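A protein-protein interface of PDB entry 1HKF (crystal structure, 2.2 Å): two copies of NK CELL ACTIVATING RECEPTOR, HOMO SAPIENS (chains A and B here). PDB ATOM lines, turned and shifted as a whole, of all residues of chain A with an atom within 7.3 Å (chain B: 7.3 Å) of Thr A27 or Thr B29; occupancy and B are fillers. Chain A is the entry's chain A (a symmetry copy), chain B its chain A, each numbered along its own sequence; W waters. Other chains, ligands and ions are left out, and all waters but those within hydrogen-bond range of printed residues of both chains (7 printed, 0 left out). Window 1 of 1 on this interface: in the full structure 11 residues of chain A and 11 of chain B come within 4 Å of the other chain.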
ATOM      1  N   SER A  22     -15.392   4.430 -16.419  1.00  0.00           N
ATOM      2  CA  SER A  22     -16.658   4.517 -15.684  1.00  0.00           C
ATOM      3  C   SER A  22     -17.790   4.466 -16.711  1.00  0.00           C
ATOM      4  O   SER A  22     -17.548   4.132 -17.859  1.00  0.00           O
ATOM      5  CB  SER A  22     -16.757   5.841 -14.918  1.00  0.00           C
ATOM      6  OG  SER A  22     -17.820   5.818 -13.978  1.00  0.00           O
ATOM      7  N   VAL A  23     -19.013   4.799 -16.295  1.00  0.00           N
ATOM      8  CA  VAL A  23     -20.150   4.788 -17.191  1.00  0.00           C
ATOM      9  C   VAL A  23     -20.867   6.102 -17.126  1.00  0.00           C
ATOM     10  O   VAL A  23     -20.748   6.834 -16.143  1.00  0.00           O
ATOM     11  CB  VAL A  23     -21.124   3.597 -16.897  1.00  0.00           C
ATOM     12  CG1 VAL A  23     -20.378   2.269 -17.116  1.00  0.00           C
ATOM     13  CG2 VAL A  23     -21.683   3.650 -15.499  1.00  0.00           C
ATOM     14  N   ALA A  24     -21.595   6.420 -18.195  1.00  0.00           N
ATOM     15  CA  ALA A  24     -22.286   7.670 -18.305  1.00  0.00           C
ATOM     16  C   ALA A  24     -23.166   7.942 -17.099  1.00  0.00           C
ATOM     17  O   ALA A  24     -23.751   7.033 -16.513  1.00  0.00           O
ATOM     18  CB  ALA A  24     -23.066   7.705 -19.580  1.00  0.00           C
ATOM     19  N   GLY A  25     -23.230   9.210 -16.707  1.00  0.00           N
ATOM     20  CA  GLY A  25     -23.981   9.590 -15.533  1.00  0.00           C
ATOM     21  C   GLY A  25     -23.113   9.540 -14.289  1.00  0.00           C
ATOM     22  O   GLY A  25     -23.378  10.283 -13.360  1.00  0.00           O
ATOM     23  N   GLN A  26     -22.086   8.679 -14.213  1.00  0.00           N
ATOM     24  CA  GLN A  26     -21.312   8.660 -12.983  1.00  0.00           C
ATOM     25  C   GLN A  26     -20.451   9.880 -12.783  1.00  0.00           C
ATOM     26  O   GLN A  26     -20.366  10.762 -13.647  1.00  0.00           O
ATOM     27  CB  GLN A  26     -20.415   7.447 -12.911  1.00  0.00           C
ATOM     28  CG  GLN A  26     -21.154   6.162 -13.049  1.00  0.00           C
ATOM     29  CD  GLN A  26     -21.915   5.813 -11.806  1.00  0.00           C
ATOM     30  OE1 GLN A  26     -21.353   5.771 -10.702  1.00  0.00           O
ATOM     31  NE2 GLN A  26     -23.189   5.540 -11.973  1.00  0.00           N
ATOM     32  N   THR A  27     -19.833   9.917 -11.610  1.00  0.00           N
ATOM     33  CA  THR A  27     -18.924  10.991 -11.237  1.00  0.00           C
ATOM     34  C   THR A  27     -17.517  10.428 -11.118  1.00  0.00           C
ATOM     35  O   THR A  27     -17.303   9.356 -10.529  1.00  0.00           O
ATOM     36  CB  THR A  27     -19.279  11.612  -9.885  1.00  0.00           C
ATOM     37  OG1 THR A  27     -20.415  12.471 -10.043  1.00  0.00           O
ATOM     38  CG2 THR A  27     -18.091  12.442  -9.354  1.00  0.00           C
ATOM     39  N   LEU A  28     -16.555  11.126 -11.705  1.00  0.00           N
ATOM     40  CA  LEU A  28     -15.172  10.662 -11.604  1.00  0.00           C
ATOM     41  C   LEU A  28     -14.350  11.513 -10.648  1.00  0.00           C
ATOM     42  O   LEU A  28     -14.415  12.744 -10.702  1.00  0.00           O
ATOM     43  CB  LEU A  28     -14.480  10.706 -12.942  1.00  0.00           C
ATOM     44  CG  LEU A  28     -13.078  10.146 -12.695  1.00  0.00           C
ATOM     45  CD1 LEU A  28     -13.105   8.772 -11.887  1.00  0.00           C
ATOM     46  CD2 LEU A  28     -12.454   9.997 -14.007  1.00  0.00           C
ATOM     47  N   THR A  29     -13.568  10.840  -9.809  1.00  0.00           N
ATOM     48  CA  THR A  29     -12.671  11.455  -8.834  1.00  0.00           C
ATOM     49  C   THR A  29     -11.239  11.070  -9.193  1.00  0.00           C
ATOM     50  O   THR A  29     -10.950   9.879  -9.364  1.00  0.00           O
ATOM     51  CB  THR A  29     -12.944  10.882  -7.465  1.00  0.00           C
ATOM     52  OG1 THR A  29     -14.312  11.151  -7.124  1.00  0.00           O
ATOM     53  CG2 THR A  29     -12.062  11.479  -6.437  1.00  0.00           C
ATOM     54  N   ARG A  72     -19.131  21.257 -14.648  1.00  0.00           N
ATOM     55  CA  ARG A  72     -19.034  19.863 -14.182  1.00  0.00           C
ATOM     56  C   ARG A  72     -17.700  19.496 -13.514  1.00  0.00           C
ATOM     57  O   ARG A  72     -17.581  18.428 -12.890  1.00  0.00           O
ATOM     58  CB  ARG A  72     -19.339  18.933 -15.353  1.00  0.00           C
ATOM     59  CG  ARG A  72     -20.474  19.365 -16.264  1.00  0.00           C
ATOM     60  CD  ARG A  72     -20.467  18.615 -17.595  1.00  0.00           C
ATOM     61  NE  ARG A  72     -19.956  17.254 -17.465  1.00  0.00           N
ATOM     62  CZ  ARG A  72     -19.126  16.671 -18.303  1.00  0.00           C
ATOM     63  NH1 ARG A  72     -18.682  17.323 -19.368  1.00  0.00           N
ATOM     64  NH2 ARG A  72     -18.730  15.412 -18.075  1.00  0.00           N
ATOM     65  N   VAL A  86      -9.419  16.045  -8.367  1.00  0.00           N
ATOM     66  CA  VAL A  86     -10.263  16.565  -9.428  1.00  0.00           C
ATOM     67  C   VAL A  86     -11.598  15.743  -9.414  1.00  0.00           C
ATOM     68  O   VAL A  86     -11.581  14.517  -9.255  1.00  0.00           O
ATOM     69  CB  VAL A  86      -9.611  16.336 -10.806  1.00  0.00           C
ATOM     70  CG1 VAL A  86     -10.536  16.858 -11.951  1.00  0.00           C
ATOM     71  CG2 VAL A  86      -8.245  17.049 -10.840  1.00  0.00           C
ATOM     72  N   THR A  87     -12.735  16.415  -9.585  1.00  0.00           N
ATOM     73  CA  THR A  87     -14.039  15.740  -9.661  1.00  0.00           C
ATOM     74  C   THR A  87     -14.676  16.151 -10.985  1.00  0.00           C
ATOM     75  O   THR A  87     -14.656  17.313 -11.336  1.00  0.00           O
ATOM     76  CB  THR A  87     -14.960  16.117  -8.485  1.00  0.00           C
ATOM     77  OG1 THR A  87     -14.360  15.701  -7.250  1.00  0.00           O
ATOM     78  CG2 THR A  87     -16.302  15.363  -8.574  1.00  0.00           C
ATOM     79  N   MET A  88     -15.128  15.171 -11.766  1.00  0.00           N
ATOM     80  CA  MET A  88     -15.827  15.404 -13.043  1.00  0.00           C
ATOM     81  C   MET A  88     -17.230  14.752 -12.846  1.00  0.00           C
ATOM     82  O   MET A  88     -17.350  13.541 -12.586  1.00  0.00           O
ATOM     83  CB  MET A  88     -15.147  14.663 -14.187  1.00  0.00           C
ATOM     84  CG  MET A  88     -13.921  15.319 -14.765  1.00  0.00           C
ATOM     85  SD  MET A  88     -13.316  14.293 -16.137  1.00  0.00           S
ATOM     86  CE  MET A  88     -14.043  15.104 -17.478  1.00  0.00           C
ATOM     87  N   THR A  89     -18.272  15.537 -12.904  1.00  0.00           N
ATOM     88  CA  THR A  89     -19.590  14.959 -12.647  1.00  0.00           C
ATOM     89  C   THR A  89     -20.334  14.768 -13.938  1.00  0.00           C
ATOM     90  O   THR A  89     -19.947  15.326 -15.028  1.00  0.00           O
ATOM     91  CB  THR A  89     -20.481  15.837 -11.706  1.00  0.00           C
ATOM     92  OG1 THR A  89     -20.736  17.069 -12.333  1.00  0.00           O
ATOM     93  CG2 THR A  89     -19.813  16.131 -10.403  1.00  0.00           C
ATOM     94  N   ASP A  90     -21.339  13.894 -13.849  1.00  0.00           N
ATOM     95  CA  ASP A  90     -22.178  13.644 -15.001  1.00  0.00           C
ATOM     96  C   ASP A  90     -21.403  13.215 -16.243  1.00  0.00           C
ATOM     97  O   ASP A  90     -21.558  13.809 -17.320  1.00  0.00           O
ATOM     98  CB  ASP A  90     -22.961  14.917 -15.339  1.00  0.00           C
ATOM     99  CG  ASP A  90     -24.094  14.634 -16.310  1.00  0.00           C
ATOM    100  OD1 ASP A  90     -24.760  13.557 -16.124  1.00  0.00           O
ATOM    101  OD2 ASP A  90     -24.299  15.454 -17.259  1.00  0.00           O
ATOM    102  N   LEU A  91     -20.562  12.197 -16.115  1.00  0.00           N
ATOM    103  CA  LEU A  91     -19.772  11.764 -17.273  1.00  0.00           C
ATOM    104  C   LEU A  91     -20.658  11.408 -18.473  1.00  0.00           C
ATOM    105  O   LEU A  91     -21.738  10.837 -18.304  1.00  0.00           O
ATOM    106  CB  LEU A  91     -18.892  10.549 -16.922  1.00  0.00           C
ATOM    107  CG  LEU A  91     -17.848  10.852 -15.826  1.00  0.00           C
ATOM    108  CD1 LEU A  91     -17.190   9.578 -15.242  1.00  0.00           C
ATOM    109  CD2 LEU A  91     -16.828  11.832 -16.428  1.00  0.00           C
ATOM    110  N   LEU B  20     -15.860  -0.845 -13.677  1.00  0.00           N
ATOM    111  CA  LEU B  20     -15.314   0.414 -13.128  1.00  0.00           C
ATOM    112  C   LEU B  20     -13.818   0.143 -13.015  1.00  0.00           C
ATOM    113  O   LEU B  20     -13.419  -0.906 -12.568  1.00  0.00           O
ATOM    114  CB  LEU B  20     -15.877   0.677 -11.732  1.00  0.00           C
ATOM    115  CG  LEU B  20     -17.408   0.797 -11.699  1.00  0.00           C
ATOM    116  CD1 LEU B  20     -17.767   1.282 -10.341  1.00  0.00           C
ATOM    117  CD2 LEU B  20     -17.917   1.791 -12.730  1.00  0.00           C
ATOM    118  N   THR B  27      -9.562   7.127  -5.227  1.00  0.00           N
ATOM    119  CA  THR B  27     -10.851   7.043  -4.556  1.00  0.00           C
ATOM    120  C   THR B  27     -11.926   6.741  -5.587  1.00  0.00           C
ATOM    121  O   THR B  27     -11.959   7.341  -6.674  1.00  0.00           O
ATOM    122  CB  THR B  27     -11.238   8.354  -3.870  1.00  0.00           C
ATOM    123  OG1 THR B  27     -10.485   8.494  -2.659  1.00  0.00           O
ATOM    124  CG2 THR B  27     -12.743   8.351  -3.529  1.00  0.00           C
ATOM    125  N   LEU B  28     -12.790   5.786  -5.271  1.00  0.00           N
ATOM    126  CA  LEU B  28     -13.871   5.463  -6.201  1.00  0.00           C
ATOM    127  C   LEU B  28     -15.218   5.979  -5.716  1.00  0.00           C
ATOM    128  O   LEU B  28     -15.560   5.810  -4.542  1.00  0.00           O
ATOM    129  CB  LEU B  28     -14.009   3.974  -6.386  1.00  0.00           C
ATOM    130  CG  LEU B  28     -15.126   3.794  -7.416  1.00  0.00           C
ATOM    131  CD1 LEU B  28     -14.925   4.714  -8.701  1.00  0.00           C
ATOM    132  CD2 LEU B  28     -15.148   2.373  -7.758  1.00  0.00           C
ATOM    133  N   THR B  29     -15.969   6.574  -6.637  1.00  0.00           N
ATOM    134  CA  THR B  29     -17.307   7.109  -6.399  1.00  0.00           C
ATOM    135  C   THR B  29     -18.293   6.331  -7.266  1.00  0.00           C
ATOM    136  O   THR B  29     -18.079   6.211  -8.479  1.00  0.00           O
ATOM    137  CB  THR B  29     -17.366   8.545  -6.858  1.00  0.00           C
ATOM    138  OG1 THR B  29     -16.390   9.298  -6.123  1.00  0.00           O
ATOM    139  CG2 THR B  29     -18.704   9.137  -6.633  1.00  0.00           C
ATOM    140  N   VAL B  30     -19.369   5.800  -6.667  1.00  0.00           N
ATOM    141  CA  VAL B  30     -20.400   5.093  -7.449  1.00  0.00           C
ATOM    142  C   VAL B  30     -21.799   5.663  -7.131  1.00  0.00           C
ATOM    143  O   VAL B  30     -22.234   5.687  -5.967  1.00  0.00           O
ATOM    144  CB  VAL B  30     -20.426   3.582  -7.125  1.00  0.00           C
ATOM    145  CG1 VAL B  30     -21.481   2.869  -7.977  1.00  0.00           C
ATOM    146  CG2 VAL B  30     -19.080   2.957  -7.407  1.00  0.00           C
ATOM    147  N   ARG B  31     -22.493   6.146  -8.151  1.00  0.00           N
ATOM    148  CA  ARG B  31     -23.834   6.657  -7.974  1.00  0.00           C
ATOM    149  C   ARG B  31     -24.883   5.605  -8.432  1.00  0.00           C
ATOM    150  O   ARG B  31     -24.726   4.976  -9.506  1.00  0.00           O
ATOM    151  CB  ARG B  31     -24.035   7.894  -8.813  1.00  0.00           C
ATOM    152  CG  ARG B  31     -23.730   9.129  -8.093  1.00  0.00           C
ATOM    153  CD  ARG B  31     -23.142  10.094  -9.064  1.00  0.00           C
ATOM    154  NE  ARG B  31     -24.163  10.938  -9.677  1.00  0.00           N
ATOM    155  CZ  ARG B  31     -24.391  12.187  -9.277  1.00  0.00           C
ATOM    156  NH1 ARG B  31     -23.682  12.702  -8.269  1.00  0.00           N
ATOM    157  NH2 ARG B  31     -25.279  12.941  -9.904  1.00  0.00           N
ATOM    158  N   TRP B  46     -23.969  -1.391  -0.072  1.00  0.00           N
ATOM    159  CA  TRP B  46     -22.909  -1.652  -1.055  1.00  0.00           C
ATOM    160  C   TRP B  46     -22.262  -2.940  -0.549  1.00  0.00           C
ATOM    161  O   TRP B  46     -21.899  -3.038   0.623  1.00  0.00           O
ATOM    162  CB  TRP B  46     -21.866  -0.529  -1.051  1.00  0.00           C
ATOM    163  CG  TRP B  46     -20.661  -0.702  -2.025  1.00  0.00           C
ATOM    164  CD1 TRP B  46     -19.324  -0.806  -1.668  1.00  0.00           C
ATOM    165  CD2 TRP B  46     -20.679  -0.630  -3.470  1.00  0.00           C
ATOM    166  NE1 TRP B  46     -18.525  -0.789  -2.791  1.00  0.00           N
ATOM    167  CE2 TRP B  46     -19.319  -0.683  -3.909  1.00  0.00           C
ATOM    168  CE3 TRP B  46     -21.711  -0.520  -4.439  1.00  0.00           C
ATOM    169  CZ2 TRP B  46     -18.959  -0.629  -5.270  1.00  0.00           C
ATOM    170  CZ3 TRP B  46     -21.365  -0.467  -5.783  1.00  0.00           C
ATOM    171  CH2 TRP B  46     -19.974  -0.519  -6.193  1.00  0.00           C
ATOM    172  N   PHE B  83     -30.890   9.554  -5.594  1.00  0.00           N
ATOM    173  CA  PHE B  83     -29.766   8.614  -5.752  1.00  0.00           C
ATOM    174  C   PHE B  83     -28.914   8.682  -4.541  1.00  0.00           C
ATOM    175  O   PHE B  83     -29.042   9.635  -3.769  1.00  0.00           O
ATOM    176  CB  PHE B  83     -28.888   8.961  -6.979  1.00  0.00           C
ATOM    177  CG  PHE B  83     -28.146  10.287  -6.860  1.00  0.00           C
ATOM    178  CD1 PHE B  83     -28.721  11.470  -7.306  1.00  0.00           C
ATOM    179  CD2 PHE B  83     -26.860  10.335  -6.307  1.00  0.00           C
ATOM    180  CE1 PHE B  83     -28.024  12.723  -7.214  1.00  0.00           C
ATOM    181  CE2 PHE B  83     -26.148  11.538  -6.200  1.00  0.00           C
ATOM    182  CZ  PHE B  83     -26.727  12.740  -6.654  1.00  0.00           C
ATOM    183  N   THR B  85     -24.702   7.815  -3.228  1.00  0.00           N
ATOM    184  CA  THR B  85     -23.356   7.734  -3.750  1.00  0.00           C
ATOM    185  C   THR B  85     -22.504   6.961  -2.795  1.00  0.00           C
ATOM    186  O   THR B  85     -22.442   7.310  -1.622  1.00  0.00           O
ATOM    187  CB  THR B  85     -22.687   9.120  -3.822  1.00  0.00           C
ATOM    188  OG1 THR B  85     -23.440   9.981  -4.693  1.00  0.00           O
ATOM    189  CG2 THR B  85     -21.264   8.959  -4.359  1.00  0.00           C
ATOM    190  N   VAL B  86     -21.862   5.914  -3.287  1.00  0.00           N
ATOM    191  CA  VAL B  86     -20.925   5.150  -2.483  1.00  0.00           C
ATOM    192  C   VAL B  86     -19.489   5.711  -2.772  1.00  0.00           C
ATOM    193  O   VAL B  86     -19.144   5.994  -3.925  1.00  0.00           O
ATOM    194  CB  VAL B  86     -20.921   3.668  -2.909  1.00  0.00           C
ATOM    195  CG1 VAL B  86     -19.883   2.854  -2.071  1.00  0.00           C
ATOM    196  CG2 VAL B  86     -22.338   3.091  -2.732  1.00  0.00           C
ATOM    197  N   THR B  87     -18.668   5.860  -1.735  1.00  0.00           N
ATOM    198  CA  THR B  87     -17.277   6.310  -1.897  1.00  0.00           C
ATOM    199  C   THR B  87     -16.389   5.243  -1.264  1.00  0.00           C
ATOM    200  O   THR B  87     -16.675   4.775  -0.181  1.00  0.00           O
ATOM    201  CB  THR B  87     -17.026   7.677  -1.233  1.00  0.00           C
ATOM    202  OG1 THR B  87     -17.848   8.674  -1.856  1.00  0.00           O
ATOM    203  CG2 THR B  87     -15.570   8.137  -1.454  1.00  0.00           C
ATOM    204  N   MET B  88     -15.383   4.780  -2.005  1.00  0.00           N
ATOM    205  CA  MET B  88     -14.397   3.798  -1.517  1.00  0.00           C
ATOM    206  C   MET B  88     -13.025   4.534  -1.626  1.00  0.00           C
ATOM    207  O   MET B  88     -12.603   4.957  -2.717  1.00  0.00           O
ATOM    208  CB  MET B  88     -14.327   2.585  -2.434  1.00  0.00           C
ATOM    209  CG  MET B  88     -15.408   1.553  -2.252  1.00  0.00           C
ATOM    210  SD  MET B  88     -15.095   0.185  -3.405  1.00  0.00           S
ATOM    211  CE  MET B  88     -14.257  -0.913  -2.367  1.00  0.00           C
ATOM    212  N   LEU B  91      -8.089   2.908  -2.767  1.00  0.00           N
ATOM    213  CA  LEU B  91      -8.215   1.608  -3.435  1.00  0.00           C
ATOM    214  C   LEU B  91      -6.893   0.829  -3.432  1.00  0.00           C
ATOM    215  O   LEU B  91      -5.821   1.419  -3.581  1.00  0.00           O
ATOM    216  CB  LEU B  91      -8.693   1.775  -4.891  1.00  0.00           C
ATOM    217  CG  LEU B  91     -10.096   2.410  -4.999  1.00  0.00           C
ATOM    218  CD1 LEU B  91     -10.445   2.877  -6.433  1.00  0.00           C
ATOM    219  CD2 LEU B  91     -11.100   1.389  -4.440  1.00  0.00           C
HETATM  220  O   HOH W   1     -22.571  12.109 -11.743  1.00  0.00           O
HETATM  221  O   HOH W   2     -17.100   6.812 -11.739  1.00  0.00           O
HETATM  222  O   HOH W   3     -20.154   8.364  -9.462  1.00  0.00           O
HETATM  223  O   HOH W   4     -10.838   6.434  -9.103  1.00  0.00           O
HETATM  224  O   HOH W   5      -9.525   9.419  -6.595  1.00  0.00           O
HETATM  225  O   HOH W   6     -18.012   4.505 -10.984  1.00  0.00           O
HETATM  226  O   HOH W   7     -21.300  13.701  -7.266  1.00  0.00           O
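OG1 of Thr B29 lies within hydrogen-bond range of OG1 of Thr A29, at 3.0 Å.
N of Arg B31 is in hydrogen-bond range of OE1 of Gln A26 (2.8 Å).
N of Val B86 is in hydrogen-bond range of O of Val B30 (2.7 Å).
The backbone NH (N) of Gly A25 lies within hydrogen-bond range of the backbone carbonyl oxygen (O) of Leu A91, at 2.7 Å.
O of Gln A26 sits at hydrogen-bond distance from N of Asp A90.
O of Gln A26 is in hydrogen-bond range of N of Leu A91, at 2.9 Å.
Among the printed residues, pairs that only touch across the chains: Gln A26 with Val B30 (3.5 Å), Thr A27 with Arg B31 (3.7 Å), Thr A29 with Thr B27 (3.8 Å), Thr A27 with Thr B29 (3.8 Å), Gly A25 with Arg B31 (3.8 Å) and Gln A26 with Thr B29 (3.98 Å).
Printed residues of chain B within 4 Å of Gly A25: Arg B31 (3.8 Å).
Of chain B, only Thr B29 (3.8 Å) and Arg B31 (3.7 Å) come within 4 Å of Thr A27.
Of the printed residues of chain B, Thr A29 touches Thr B27 and Thr B29.
Printed residues of chain A within 4 Å of Thr B27: Thr A29.
Printed residues of chain A within 4 Å of Thr B29: Gln A26 (3.98 Å), Thr A27 (3.8 Å) and Thr A29 (3.0 Å).
Of the printed residues of chain A, Val B30 touches Gln A26.
Of the printed residues of chain A, Arg B31 touches Gly A25, Gln A26 and Thr A27.
The nearest residue of chain B that does not touch Thr A27 is Leu B28 (5.5 Å).
The nearest printed residue of chain A that does not touch Thr B29 is Leu A28 (5.4 Å).
Of the 13 printed residues of chain B, 4 touch a printed residue of chain A.
Hydrophobic or aromatic side chains of chain B within 4 Å of the printed part of chain A: Val B30.
Along chain A the printed residues that touch a printed residue of chain B span positions 25 to 29.
Among the printed residues, 8 pairs touch across the chains.
Thr A27 touches Thr B29, and with the chains exchanged Thr A29 touches Thr B27.
Thr A29 touches its own counterpart, Thr B29.
Water W2 lies within hydrogen-bond range of the side-chain hydroxyl of Ser A22 (2.6 Å), the backbone carbonyl oxygen of Thr A27 (2.8 Å) and the backbone carbonyl oxygen of Thr B29 (3.5 Å).
Water W1 lies within hydrogen-bond range of the backbone carbonyl oxygen of Gly A25 (2.6 Å), the side-chain hydroxyl of Thr A27 (2.8 Å), the guanidinium group of Arg B31 (2.9 Å), the backbone NH of Asp A90 (3.0 Å) and the backbone carbonyl oxygen of Gln A26 (3.2 Å).
Water W5 lies within hydrogen-bond range of N of Thr B27 (2.7 Å) and O of Thr A29 (3.1 Å).
Water W3 lies within hydrogen-bond range of N of Thr A27 (2.7 Å), OE1 of Gln A26 (3.1 Å), O of Thr B29 (3.1 Å) and N of Arg B31 (3.5 Å).
Water W4 lies within hydrogen-bond range of the backbone carbonyl oxygen of Thr B27 (2.8 Å) and the backbone carbonyl oxygen of Thr A29 (3.5 Å).
Water W6 bridges the backbone carbonyl oxygen of Thr B29 (3.0 Å) and the side-chain hydroxyl of Ser A22 (3.3 Å).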
